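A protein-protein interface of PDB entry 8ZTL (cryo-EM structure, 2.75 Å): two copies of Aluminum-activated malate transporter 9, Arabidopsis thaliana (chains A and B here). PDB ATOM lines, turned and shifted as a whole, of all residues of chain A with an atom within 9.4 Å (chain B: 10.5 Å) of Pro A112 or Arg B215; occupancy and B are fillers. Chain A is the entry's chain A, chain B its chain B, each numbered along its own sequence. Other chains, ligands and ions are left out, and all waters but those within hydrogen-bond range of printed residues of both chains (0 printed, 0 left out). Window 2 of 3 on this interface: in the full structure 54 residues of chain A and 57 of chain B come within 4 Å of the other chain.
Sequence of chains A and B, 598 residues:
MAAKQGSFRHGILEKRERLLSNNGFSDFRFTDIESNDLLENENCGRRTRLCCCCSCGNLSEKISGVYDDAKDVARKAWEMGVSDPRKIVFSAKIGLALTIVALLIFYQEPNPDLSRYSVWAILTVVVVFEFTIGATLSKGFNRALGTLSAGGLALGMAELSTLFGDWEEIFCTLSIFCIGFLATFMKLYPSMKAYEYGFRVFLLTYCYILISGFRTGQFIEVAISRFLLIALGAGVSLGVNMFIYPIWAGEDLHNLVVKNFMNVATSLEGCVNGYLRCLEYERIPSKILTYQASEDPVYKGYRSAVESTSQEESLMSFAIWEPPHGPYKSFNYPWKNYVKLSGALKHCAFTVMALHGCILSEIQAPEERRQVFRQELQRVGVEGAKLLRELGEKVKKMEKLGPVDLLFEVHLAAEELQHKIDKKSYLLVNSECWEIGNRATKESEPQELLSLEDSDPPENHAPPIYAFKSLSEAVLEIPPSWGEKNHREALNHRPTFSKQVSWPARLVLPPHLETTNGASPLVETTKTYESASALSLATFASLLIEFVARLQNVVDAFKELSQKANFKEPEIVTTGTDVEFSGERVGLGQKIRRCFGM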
ATOM      1  N   ILE A 105     -20.797 -23.936  28.504  1.00  0.00           N
ATOM      2  CA  ILE A 105     -20.960 -22.496  28.711  1.00  0.00           C
ATOM      3  C   ILE A 105     -22.092 -21.950  27.844  1.00  0.00           C
ATOM      4  O   ILE A 105     -22.917 -21.153  28.304  1.00  0.00           O
ATOM      5  CB  ILE A 105     -19.638 -21.753  28.446  1.00  0.00           C
ATOM      6  CG1 ILE A 105     -18.520 -22.305  29.328  1.00  0.00           C
ATOM      7  CG2 ILE A 105     -19.804 -20.264  28.678  1.00  0.00           C
ATOM      8  CD1 ILE A 105     -17.179 -21.662  29.067  1.00  0.00           C
ATOM      9  N   PHE A 106     -22.147 -22.374  26.581  1.00  0.00           N
ATOM     10  CA  PHE A 106     -23.141 -21.846  25.652  1.00  0.00           C
ATOM     11  C   PHE A 106     -24.554 -22.203  26.087  1.00  0.00           C
ATOM     12  O   PHE A 106     -25.412 -21.322  26.218  1.00  0.00           O
ATOM     13  CB  PHE A 106     -22.870 -22.357  24.237  1.00  0.00           C
ATOM     14  CG  PHE A 106     -21.738 -21.652  23.546  1.00  0.00           C
ATOM     15  CD1 PHE A 106     -21.485 -20.313  23.793  1.00  0.00           C
ATOM     16  CD2 PHE A 106     -20.931 -22.325  22.646  1.00  0.00           C
ATOM     17  CE1 PHE A 106     -20.448 -19.664  23.160  1.00  0.00           C
ATOM     18  CE2 PHE A 106     -19.894 -21.680  22.011  1.00  0.00           C
ATOM     19  CZ  PHE A 106     -19.652 -20.347  22.268  1.00  0.00           C
ATOM     20  N   TYR A 107     -24.822 -23.483  26.331  1.00  0.00           N
ATOM     21  CA  TYR A 107     -26.166 -23.896  26.730  1.00  0.00           C
ATOM     22  C   TYR A 107     -26.237 -23.841  28.249  1.00  0.00           C
ATOM     23  O   TYR A 107     -25.711 -24.710  28.945  1.00  0.00           O
ATOM     24  CB  TYR A 107     -26.499 -25.281  26.187  1.00  0.00           C
ATOM     25  CG  TYR A 107     -26.462 -25.360  24.678  1.00  0.00           C
ATOM     26  CD1 TYR A 107     -25.280 -25.618  24.001  1.00  0.00           C
ATOM     27  CD2 TYR A 107     -27.614 -25.171  23.930  1.00  0.00           C
ATOM     28  CE1 TYR A 107     -25.248 -25.689  22.623  1.00  0.00           C
ATOM     29  CE2 TYR A 107     -27.591 -25.239  22.552  1.00  0.00           C
ATOM     30  CZ  TYR A 107     -26.407 -25.498  21.904  1.00  0.00           C
ATOM     31  OH  TYR A 107     -26.382 -25.566  20.529  1.00  0.00           O
ATOM     32  N   GLN A 108     -26.886 -22.797  28.759  1.00  0.00           N
ATOM     33  CA  GLN A 108     -27.000 -22.557  30.188  1.00  0.00           C
ATOM     34  C   GLN A 108     -28.433 -22.160  30.507  1.00  0.00           C
ATOM     35  O   GLN A 108     -29.215 -21.816  29.618  1.00  0.00           O
ATOM     36  CB  GLN A 108     -26.025 -21.466  30.655  1.00  0.00           C
ATOM     37  CG  GLN A 108     -25.007 -21.944  31.675  1.00  0.00           C
ATOM     38  CD  GLN A 108     -24.202 -20.809  32.278  1.00  0.00           C
ATOM     39  OE1 GLN A 108     -23.650 -19.975  31.560  1.00  0.00           O
ATOM     40  NE2 GLN A 108     -24.129 -20.773  33.605  1.00  0.00           N
ATOM     41  N   GLU A 109     -28.766 -22.226  31.791  1.00  0.00           N
ATOM     42  CA  GLU A 109     -30.074 -21.787  32.255  1.00  0.00           C
ATOM     43  C   GLU A 109     -30.431 -20.447  31.615  1.00  0.00           C
ATOM     44  O   GLU A 109     -29.572 -19.561  31.517  1.00  0.00           O
ATOM     45  CB  GLU A 109     -30.091 -21.658  33.781  1.00  0.00           C
ATOM     46  CG  GLU A 109     -29.212 -20.543  34.334  1.00  0.00           C
ATOM     47  CD  GLU A 109     -27.746 -20.720  33.995  1.00  0.00           C
ATOM     48  OE1 GLU A 109     -27.221 -21.835  34.193  1.00  0.00           O
ATOM     49  OE2 GLU A 109     -27.119 -19.745  33.532  1.00  0.00           O
ATOM     50  N   PRO A 110     -31.677 -20.266  31.159  1.00  0.00           N
ATOM     51  CA  PRO A 110     -32.053 -19.025  30.466  1.00  0.00           C
ATOM     52  C   PRO A 110     -31.488 -17.771  31.117  1.00  0.00           C
ATOM     53  O   PRO A 110     -31.120 -16.818  30.424  1.00  0.00           O
ATOM     54  CB  PRO A 110     -33.583 -19.046  30.535  1.00  0.00           C
ATOM     55  CG  PRO A 110     -33.926 -20.499  30.532  1.00  0.00           C
ATOM     56  CD  PRO A 110     -32.798 -21.221  31.234  1.00  0.00           C
ATOM     57  N   ASN A 111     -31.416 -17.761  32.439  1.00  0.00           N
ATOM     58  CA  ASN A 111     -30.835 -16.635  33.158  1.00  0.00           C
ATOM     59  C   ASN A 111     -29.322 -16.627  32.976  1.00  0.00           C
ATOM     60  O   ASN A 111     -28.638 -17.477  33.562  1.00  0.00           O
ATOM     61  CB  ASN A 111     -31.192 -16.708  34.641  1.00  0.00           C
ATOM     62  CG  ASN A 111     -32.682 -16.576  34.890  1.00  0.00           C
ATOM     63  OD1 ASN A 111     -33.272 -17.362  35.631  1.00  0.00           O
ATOM     64  ND2 ASN A 111     -33.299 -15.575  34.272  1.00  0.00           N
ATOM     65  N   PRO A 112     -28.759 -15.708  32.194  1.00  0.00           N
ATOM     66  CA  PRO A 112     -27.305 -15.693  32.006  1.00  0.00           C
ATOM     67  C   PRO A 112     -26.602 -14.886  33.085  1.00  0.00           C
ATOM     68  O   PRO A 112     -25.387 -15.011  33.275  1.00  0.00           O
ATOM     69  CB  PRO A 112     -27.146 -15.052  30.625  1.00  0.00           C
ATOM     70  CG  PRO A 112     -28.311 -14.106  30.530  1.00  0.00           C
ATOM     71  CD  PRO A 112     -29.420 -14.639  31.426  1.00  0.00           C
ATOM     72  N   ASP A 113     -27.361 -14.053  33.797  1.00  0.00           N
ATOM     73  CA  ASP A 113     -26.788 -13.235  34.856  1.00  0.00           C
ATOM     74  C   ASP A 113     -26.382 -14.053  36.073  1.00  0.00           C
ATOM     75  O   ASP A 113     -25.697 -13.522  36.953  1.00  0.00           O
ATOM     76  CB  ASP A 113     -27.778 -12.146  35.270  1.00  0.00           C
ATOM     77  CG  ASP A 113     -27.942 -11.075  34.209  1.00  0.00           C
ATOM     78  OD1 ASP A 113     -27.097 -11.012  33.291  1.00  0.00           O
ATOM     79  OD2 ASP A 113     -28.915 -10.298  34.292  1.00  0.00           O
ATOM     80  N   LEU A 114     -26.787 -15.324  36.146  1.00  0.00           N
ATOM     81  CA  LEU A 114     -26.361 -16.173  37.253  1.00  0.00           C
ATOM     82  C   LEU A 114     -24.843 -16.252  37.329  1.00  0.00           C
ATOM     83  O   LEU A 114     -24.268 -16.303  38.424  1.00  0.00           O
ATOM     84  CB  LEU A 114     -26.964 -17.569  37.106  1.00  0.00           C
ATOM     85  CG  LEU A 114     -26.585 -18.596  38.174  1.00  0.00           C
ATOM     86  CD1 LEU A 114     -26.813 -18.040  39.572  1.00  0.00           C
ATOM     87  CD2 LEU A 114     -27.359 -19.890  37.977  1.00  0.00           C
ATOM     88  N   SER A 115     -24.176 -16.265  36.178  1.00  0.00           N
ATOM     89  CA  SER A 115     -22.723 -16.281  36.139  1.00  0.00           C
ATOM     90  C   SER A 115     -22.239 -15.504  34.925  1.00  0.00           C
ATOM     91  O   SER A 115     -22.829 -15.587  33.845  1.00  0.00           O
ATOM     92  CB  SER A 115     -22.173 -17.710  36.106  1.00  0.00           C
ATOM     93  OG  SER A 115     -22.477 -18.397  37.308  1.00  0.00           O
ATOM     94  N   ARG A 116     -21.158 -14.752  35.120  1.00  0.00           N
ATOM     95  CA  ARG A 116     -20.497 -14.028  34.048  1.00  0.00           C
ATOM     96  C   ARG A 116     -19.002 -14.291  34.010  1.00  0.00           C
ATOM     97  O   ARG A 116     -18.340 -13.861  33.059  1.00  0.00           O
ATOM     98  CB  ARG A 116     -20.734 -12.517  34.188  1.00  0.00           C
ATOM     99  CG  ARG A 116     -22.194 -12.098  34.096  1.00  0.00           C
ATOM    100  CD  ARG A 116     -22.773 -12.393  32.726  1.00  0.00           C
ATOM    101  NE  ARG A 116     -22.062 -11.665  31.683  1.00  0.00           N
ATOM    102  CZ  ARG A 116     -22.292 -10.399  31.366  1.00  0.00           C
ATOM    103  NH1 ARG A 116     -23.211  -9.685  31.996  1.00  0.00           N
ATOM    104  NH2 ARG A 116     -21.581  -9.833  30.396  1.00  0.00           N
ATOM    105  N   TYR A 117     -18.454 -14.969  35.011  1.00  0.00           N
ATOM    106  CA  TYR A 117     -17.053 -15.375  35.027  1.00  0.00           C
ATOM    107  C   TYR A 117     -16.925 -16.830  34.582  1.00  0.00           C
ATOM    108  O   TYR A 117     -16.521 -17.713  35.335  1.00  0.00           O
ATOM    109  CB  TYR A 117     -16.463 -15.156  36.415  1.00  0.00           C
ATOM    110  CG  TYR A 117     -16.486 -13.708  36.841  1.00  0.00           C
ATOM    111  CD1 TYR A 117     -15.995 -12.714  36.006  1.00  0.00           C
ATOM    112  CD2 TYR A 117     -17.018 -13.330  38.066  1.00  0.00           C
ATOM    113  CE1 TYR A 117     -16.018 -11.389  36.384  1.00  0.00           C
ATOM    114  CE2 TYR A 117     -17.045 -12.004  38.453  1.00  0.00           C
ATOM    115  CZ  TYR A 117     -16.543 -11.039  37.605  1.00  0.00           C
ATOM    116  OH  TYR A 117     -16.566  -9.716  37.980  1.00  0.00           O
ATOM    117  N   SER A 118     -17.288 -17.070  33.322  1.00  0.00           N
ATOM    118  CA  SER A 118     -17.311 -18.417  32.769  1.00  0.00           C
ATOM    119  C   SER A 118     -16.100 -18.732  31.906  1.00  0.00           C
ATOM    120  O   SER A 118     -15.858 -19.908  31.616  1.00  0.00           O
ATOM    121  CB  SER A 118     -18.585 -18.633  31.945  1.00  0.00           C
ATOM    122  OG  SER A 118     -19.708 -18.055  32.584  1.00  0.00           O
ATOM    123  N   VAL A 119     -15.336 -17.720  31.489  1.00  0.00           N
ATOM    124  CA  VAL A 119     -14.126 -17.980  30.725  1.00  0.00           C
ATOM    125  C   VAL A 119     -13.048 -18.576  31.611  1.00  0.00           C
ATOM    126  O   VAL A 119     -12.078 -19.158  31.106  1.00  0.00           O
ATOM    127  CB  VAL A 119     -13.625 -16.692  30.052  1.00  0.00           C
ATOM    128  CG1 VAL A 119     -14.550 -16.299  28.917  1.00  0.00           C
ATOM    129  CG2 VAL A 119     -13.508 -15.575  31.075  1.00  0.00           C
ATOM    130  N   ALA B 158     -16.207 -14.358  14.102  1.00  0.00           N
ATOM    131  CA  ALA B 158     -17.424 -13.867  14.734  1.00  0.00           C
ATOM    132  C   ALA B 158     -18.342 -13.237  13.701  1.00  0.00           C
ATOM    133  O   ALA B 158     -19.560 -13.437  13.734  1.00  0.00           O
ATOM    134  CB  ALA B 158     -17.084 -12.868  15.836  1.00  0.00           C
ATOM    135  N   GLU B 168     -25.740 -21.077  15.257  1.00  0.00           N
ATOM    136  CA  GLU B 168     -24.722 -20.127  15.692  1.00  0.00           C
ATOM    137  C   GLU B 168     -23.727 -20.768  16.654  1.00  0.00           C
ATOM    138  O   GLU B 168     -22.514 -20.771  16.404  1.00  0.00           O
ATOM    139  CB  GLU B 168     -25.401 -18.922  16.357  1.00  0.00           C
ATOM    140  CG  GLU B 168     -24.593 -17.641  16.347  1.00  0.00           C
ATOM    141  CD  GLU B 168     -24.953 -16.745  15.181  1.00  0.00           C
ATOM    142  OE1 GLU B 168     -25.576 -17.241  14.221  1.00  0.00           O
ATOM    143  OE2 GLU B 168     -24.619 -15.544  15.229  1.00  0.00           O
ATOM    144  N   GLU B 169     -24.232 -21.339  17.750  1.00  0.00           N
ATOM    145  CA  GLU B 169     -23.359 -21.965  18.733  1.00  0.00           C
ATOM    146  C   GLU B 169     -22.665 -23.191  18.162  1.00  0.00           C
ATOM    147  O   GLU B 169     -21.513 -23.468  18.512  1.00  0.00           O
ATOM    148  CB  GLU B 169     -24.163 -22.336  19.979  1.00  0.00           C
ATOM    149  CG  GLU B 169     -25.167 -21.276  20.402  1.00  0.00           C
ATOM    150  CD  GLU B 169     -26.524 -21.459  19.748  1.00  0.00           C
ATOM    151  OE1 GLU B 169     -26.609 -22.203  18.751  1.00  0.00           O
ATOM    152  OE2 GLU B 169     -27.505 -20.853  20.227  1.00  0.00           O
ATOM    153  N   CYS B 172     -19.762 -21.875  16.057  1.00  0.00           N
ATOM    154  CA  CYS B 172     -18.707 -21.356  16.923  1.00  0.00           C
ATOM    155  C   CYS B 172     -17.935 -22.486  17.597  1.00  0.00           C
ATOM    156  O   CYS B 172     -16.698 -22.452  17.672  1.00  0.00           O
ATOM    157  CB  CYS B 172     -19.310 -20.414  17.962  1.00  0.00           C
ATOM    158  SG  CYS B 172     -19.525 -18.715  17.386  1.00  0.00           S
ATOM    159  N   TYR B 208     -10.727 -16.499  24.359  1.00  0.00           N
ATOM    160  CA  TYR B 208     -11.296 -15.421  25.155  1.00  0.00           C
ATOM    161  C   TYR B 208     -12.178 -14.522  24.305  1.00  0.00           C
ATOM    162  O   TYR B 208     -13.277 -14.143  24.727  1.00  0.00           O
ATOM    163  CB  TYR B 208     -10.188 -14.607  25.822  1.00  0.00           C
ATOM    164  CG  TYR B 208     -10.699 -13.435  26.628  1.00  0.00           C
ATOM    165  CD1 TYR B 208     -11.170 -13.611  27.921  1.00  0.00           C
ATOM    166  CD2 TYR B 208     -10.727 -12.154  26.094  1.00  0.00           C
ATOM    167  CE1 TYR B 208     -11.643 -12.547  28.660  1.00  0.00           C
ATOM    168  CE2 TYR B 208     -11.196 -11.084  26.826  1.00  0.00           C
ATOM    169  CZ  TYR B 208     -11.655 -11.287  28.107  1.00  0.00           C
ATOM    170  OH  TYR B 208     -12.127 -10.228  28.844  1.00  0.00           O
ATOM    171  N   ILE B 209     -11.730 -14.181  23.093  1.00  0.00           N
ATOM    172  CA  ILE B 209     -12.513 -13.260  22.279  1.00  0.00           C
ATOM    173  C   ILE B 209     -13.768 -13.942  21.749  1.00  0.00           C
ATOM    174  O   ILE B 209     -14.819 -13.306  21.618  1.00  0.00           O
ATOM    175  CB  ILE B 209     -11.660 -12.667  21.149  1.00  0.00           C
ATOM    176  CG1 ILE B 209     -10.739 -11.584  21.708  1.00  0.00           C
ATOM    177  CG2 ILE B 209     -12.554 -12.092  20.067  1.00  0.00           C
ATOM    178  CD1 ILE B 209      -9.755 -11.046  20.708  1.00  0.00           C
ATOM    179  N   LEU B 210     -13.688 -15.236  21.421  1.00  0.00           N
ATOM    180  CA  LEU B 210     -14.891 -15.918  20.954  1.00  0.00           C
ATOM    181  C   LEU B 210     -15.910 -16.134  22.070  1.00  0.00           C
ATOM    182  O   LEU B 210     -17.116 -16.093  21.809  1.00  0.00           O
ATOM    183  CB  LEU B 210     -14.531 -17.250  20.299  1.00  0.00           C
ATOM    184  CG  LEU B 210     -15.340 -17.557  19.036  1.00  0.00           C
ATOM    185  CD1 LEU B 210     -15.122 -16.488  17.985  1.00  0.00           C
ATOM    186  CD2 LEU B 210     -14.991 -18.925  18.485  1.00  0.00           C
ATOM    187  N   ILE B 211     -15.465 -16.358  23.310  1.00  0.00           N
ATOM    188  CA  ILE B 211     -16.412 -16.620  24.393  1.00  0.00           C
ATOM    189  C   ILE B 211     -16.912 -15.361  25.096  1.00  0.00           C
ATOM    190  O   ILE B 211     -17.986 -15.396  25.711  1.00  0.00           O
ATOM    191  CB  ILE B 211     -15.806 -17.574  25.438  1.00  0.00           C
ATOM    192  CG1 ILE B 211     -15.634 -18.973  24.850  1.00  0.00           C
ATOM    193  CG2 ILE B 211     -16.678 -17.637  26.676  1.00  0.00           C
ATOM    194  CD1 ILE B 211     -16.912 -19.545  24.284  1.00  0.00           C
ATOM    195  N   SER B 212     -16.180 -14.248  25.018  1.00  0.00           N
ATOM    196  CA  SER B 212     -16.585 -13.014  25.677  1.00  0.00           C
ATOM    197  C   SER B 212     -17.243 -12.027  24.720  1.00  0.00           C
ATOM    198  O   SER B 212     -17.325 -10.835  25.028  1.00  0.00           O
ATOM    199  CB  SER B 212     -15.383 -12.361  26.360  1.00  0.00           C
ATOM    200  OG  SER B 212     -15.094 -12.998  27.591  1.00  0.00           O
ATOM    201  N   GLY B 213     -17.707 -12.497  23.568  1.00  0.00           N
ATOM    202  CA  GLY B 213     -18.438 -11.653  22.643  1.00  0.00           C
ATOM    203  C   GLY B 213     -19.653 -12.336  22.052  1.00  0.00           C
ATOM    204  O   GLY B 213     -19.862 -12.284  20.836  1.00  0.00           O
ATOM    205  N   PHE B 214     -20.460 -12.976  22.890  1.00  0.00           N
ATOM    206  CA  PHE B 214     -21.583 -13.776  22.418  1.00  0.00           C
ATOM    207  C   PHE B 214     -22.918 -13.362  23.010  1.00  0.00           C
ATOM    208  O   PHE B 214     -23.907 -13.267  22.280  1.00  0.00           O
ATOM    209  CB  PHE B 214     -21.330 -15.259  22.737  1.00  0.00           C
ATOM    210  CG  PHE B 214     -22.335 -16.196  22.132  1.00  0.00           C
ATOM    211  CD1 PHE B 214     -23.549 -16.435  22.757  1.00  0.00           C
ATOM    212  CD2 PHE B 214     -22.058 -16.853  20.945  1.00  0.00           C
ATOM    213  CE1 PHE B 214     -24.470 -17.301  22.202  1.00  0.00           C
ATOM    214  CE2 PHE B 214     -22.976 -17.720  20.387  1.00  0.00           C
ATOM    215  CZ  PHE B 214     -24.184 -17.944  21.017  1.00  0.00           C
ATOM    216  N   ARG B 215     -22.978 -13.108  24.316  1.00  0.00           N
ATOM    217  CA  ARG B 215     -24.241 -12.778  24.961  1.00  0.00           C
ATOM    218  C   ARG B 215     -24.653 -11.329  24.753  1.00  0.00           C
ATOM    219  O   ARG B 215     -25.781 -10.966  25.104  1.00  0.00           O
ATOM    220  CB  ARG B 215     -24.151 -13.086  26.457  1.00  0.00           C
ATOM    221  CG  ARG B 215     -25.466 -12.973  27.207  1.00  0.00           C
ATOM    222  CD  ARG B 215     -25.223 -12.564  28.648  1.00  0.00           C
ATOM    223  NE  ARG B 215     -23.822 -12.718  29.019  1.00  0.00           N
ATOM    224  CZ  ARG B 215     -23.270 -13.861  29.399  1.00  0.00           C
ATOM    225  NH1 ARG B 215     -23.975 -14.977  29.476  1.00  0.00           N
ATOM    226  NH2 ARG B 215     -21.977 -13.887  29.709  1.00  0.00           N
ATOM    227  N   THR B 216     -23.779 -10.501  24.195  1.00  0.00           N
ATOM    228  CA  THR B 216     -24.061  -9.091  23.966  1.00  0.00           C
ATOM    229  C   THR B 216     -23.921  -8.674  22.513  1.00  0.00           C
ATOM    230  O   THR B 216     -24.733  -7.888  22.021  1.00  0.00           O
ATOM    231  CB  THR B 216     -23.131  -8.222  24.824  1.00  0.00           C
ATOM    232  OG1 THR B 216     -21.907  -7.991  24.115  1.00  0.00           O
ATOM    233  CG2 THR B 216     -22.819  -8.918  26.138  1.00  0.00           C
ATOM    234  N   GLY B 217     -22.911  -9.181  21.813  1.00  0.00           N
ATOM    235  CA  GLY B 217     -22.649  -8.776  20.450  1.00  0.00           C
ATOM    236  C   GLY B 217     -21.813  -7.513  20.413  1.00  0.00           C
ATOM    237  O   GLY B 217     -21.545  -6.872  21.431  1.00  0.00           O
ATOM    238  N   GLN B 218     -21.397  -7.142  19.203  1.00  0.00           N
ATOM    239  CA  GLN B 218     -20.637  -5.912  18.985  1.00  0.00           C
ATOM    240  C   GLN B 218     -19.532  -5.765  20.030  1.00  0.00           C
ATOM    241  O   GLN B 218     -19.379  -4.726  20.677  1.00  0.00           O
ATOM    242  CB  GLN B 218     -21.559  -4.691  18.980  1.00  0.00           C
ATOM    243  CG  GLN B 218     -22.555  -4.665  17.830  1.00  0.00           C
ATOM    244  CD  GLN B 218     -23.853  -5.375  18.160  1.00  0.00           C
ATOM    245  OE1 GLN B 218     -23.988  -6.580  17.943  1.00  0.00           O
ATOM    246  NE2 GLN B 218     -24.818  -4.630  18.688  1.00  0.00           N
ATOM    247  N   PHE B 219     -18.754  -6.833  20.193  1.00  0.00           N
ATOM    248  CA  PHE B 219     -17.639  -6.865  21.138  1.00  0.00           C
ATOM    249  C   PHE B 219     -16.410  -6.401  20.368  1.00  0.00           C
ATOM    250  O   PHE B 219     -15.647  -7.202  19.827  1.00  0.00           O
ATOM    251  CB  PHE B 219     -17.484  -8.276  21.699  1.00  0.00           C
ATOM    252  CG  PHE B 219     -16.207  -8.516  22.463  1.00  0.00           C
ATOM    253  CD1 PHE B 219     -16.115  -8.195  23.804  1.00  0.00           C
ATOM    254  CD2 PHE B 219     -15.107  -9.085  21.844  1.00  0.00           C
ATOM    255  CE1 PHE B 219     -14.946  -8.430  24.510  1.00  0.00           C
ATOM    256  CE2 PHE B 219     -13.938  -9.313  22.545  1.00  0.00           C
ATOM    257  CZ  PHE B 219     -13.858  -8.983  23.878  1.00  0.00           C
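The guanidinium group of Arg A116 sits close to the guanidinium group of Arg B215 (3.0 Å).
Ile B211 touches Phe A106. Phe A106 touches Phe B214. Tyr A107 touches Glu B169. Pro A112 touches Arg B215. Val A119 touches Ile B211. Ser B212 touches Val A119.
Of the printed residues of chain A, Arg B215 touches Pro A112 and Arg A116. No residue of chain B comes within 4 Å of Asp A113. No residue of chain B comes within 4 Å of Ser A115. Arg A116 touches just one residue of chain B: Arg B215 (3.0 Å). Of the printed residues of chain B, Val A119 touches Ile B211 (3.4 Å) and Ser B212 (3.6 Å). Printed residues of chain A within 4 Å of Ile B211: Phe A106 (3.5 Å) and Val A119 (3.4 Å). Printed residues of chain B within 4 Å of Tyr A107: Glu B169 (3.8 Å).
Hydrophobic or aromatic side chains of chain B within 4 Å of the printed part of chain A: Ile B211 and Phe B214. Of the 15 printed residues of chain A, 5 touch a printed residue of chain B. Hydrophobic or aromatic side chains of chain A that line the printed part of chain B: Phe A106, Tyr A107, Pro A112 and Val A119. Among the printed residues, 7 pairs touch across the chains. Among the printed residues, no Asp or Glu carboxylate lies within 4 Å of a Lys or Arg side-chain nitrogen of the other chain.
No position is printed for both chains.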
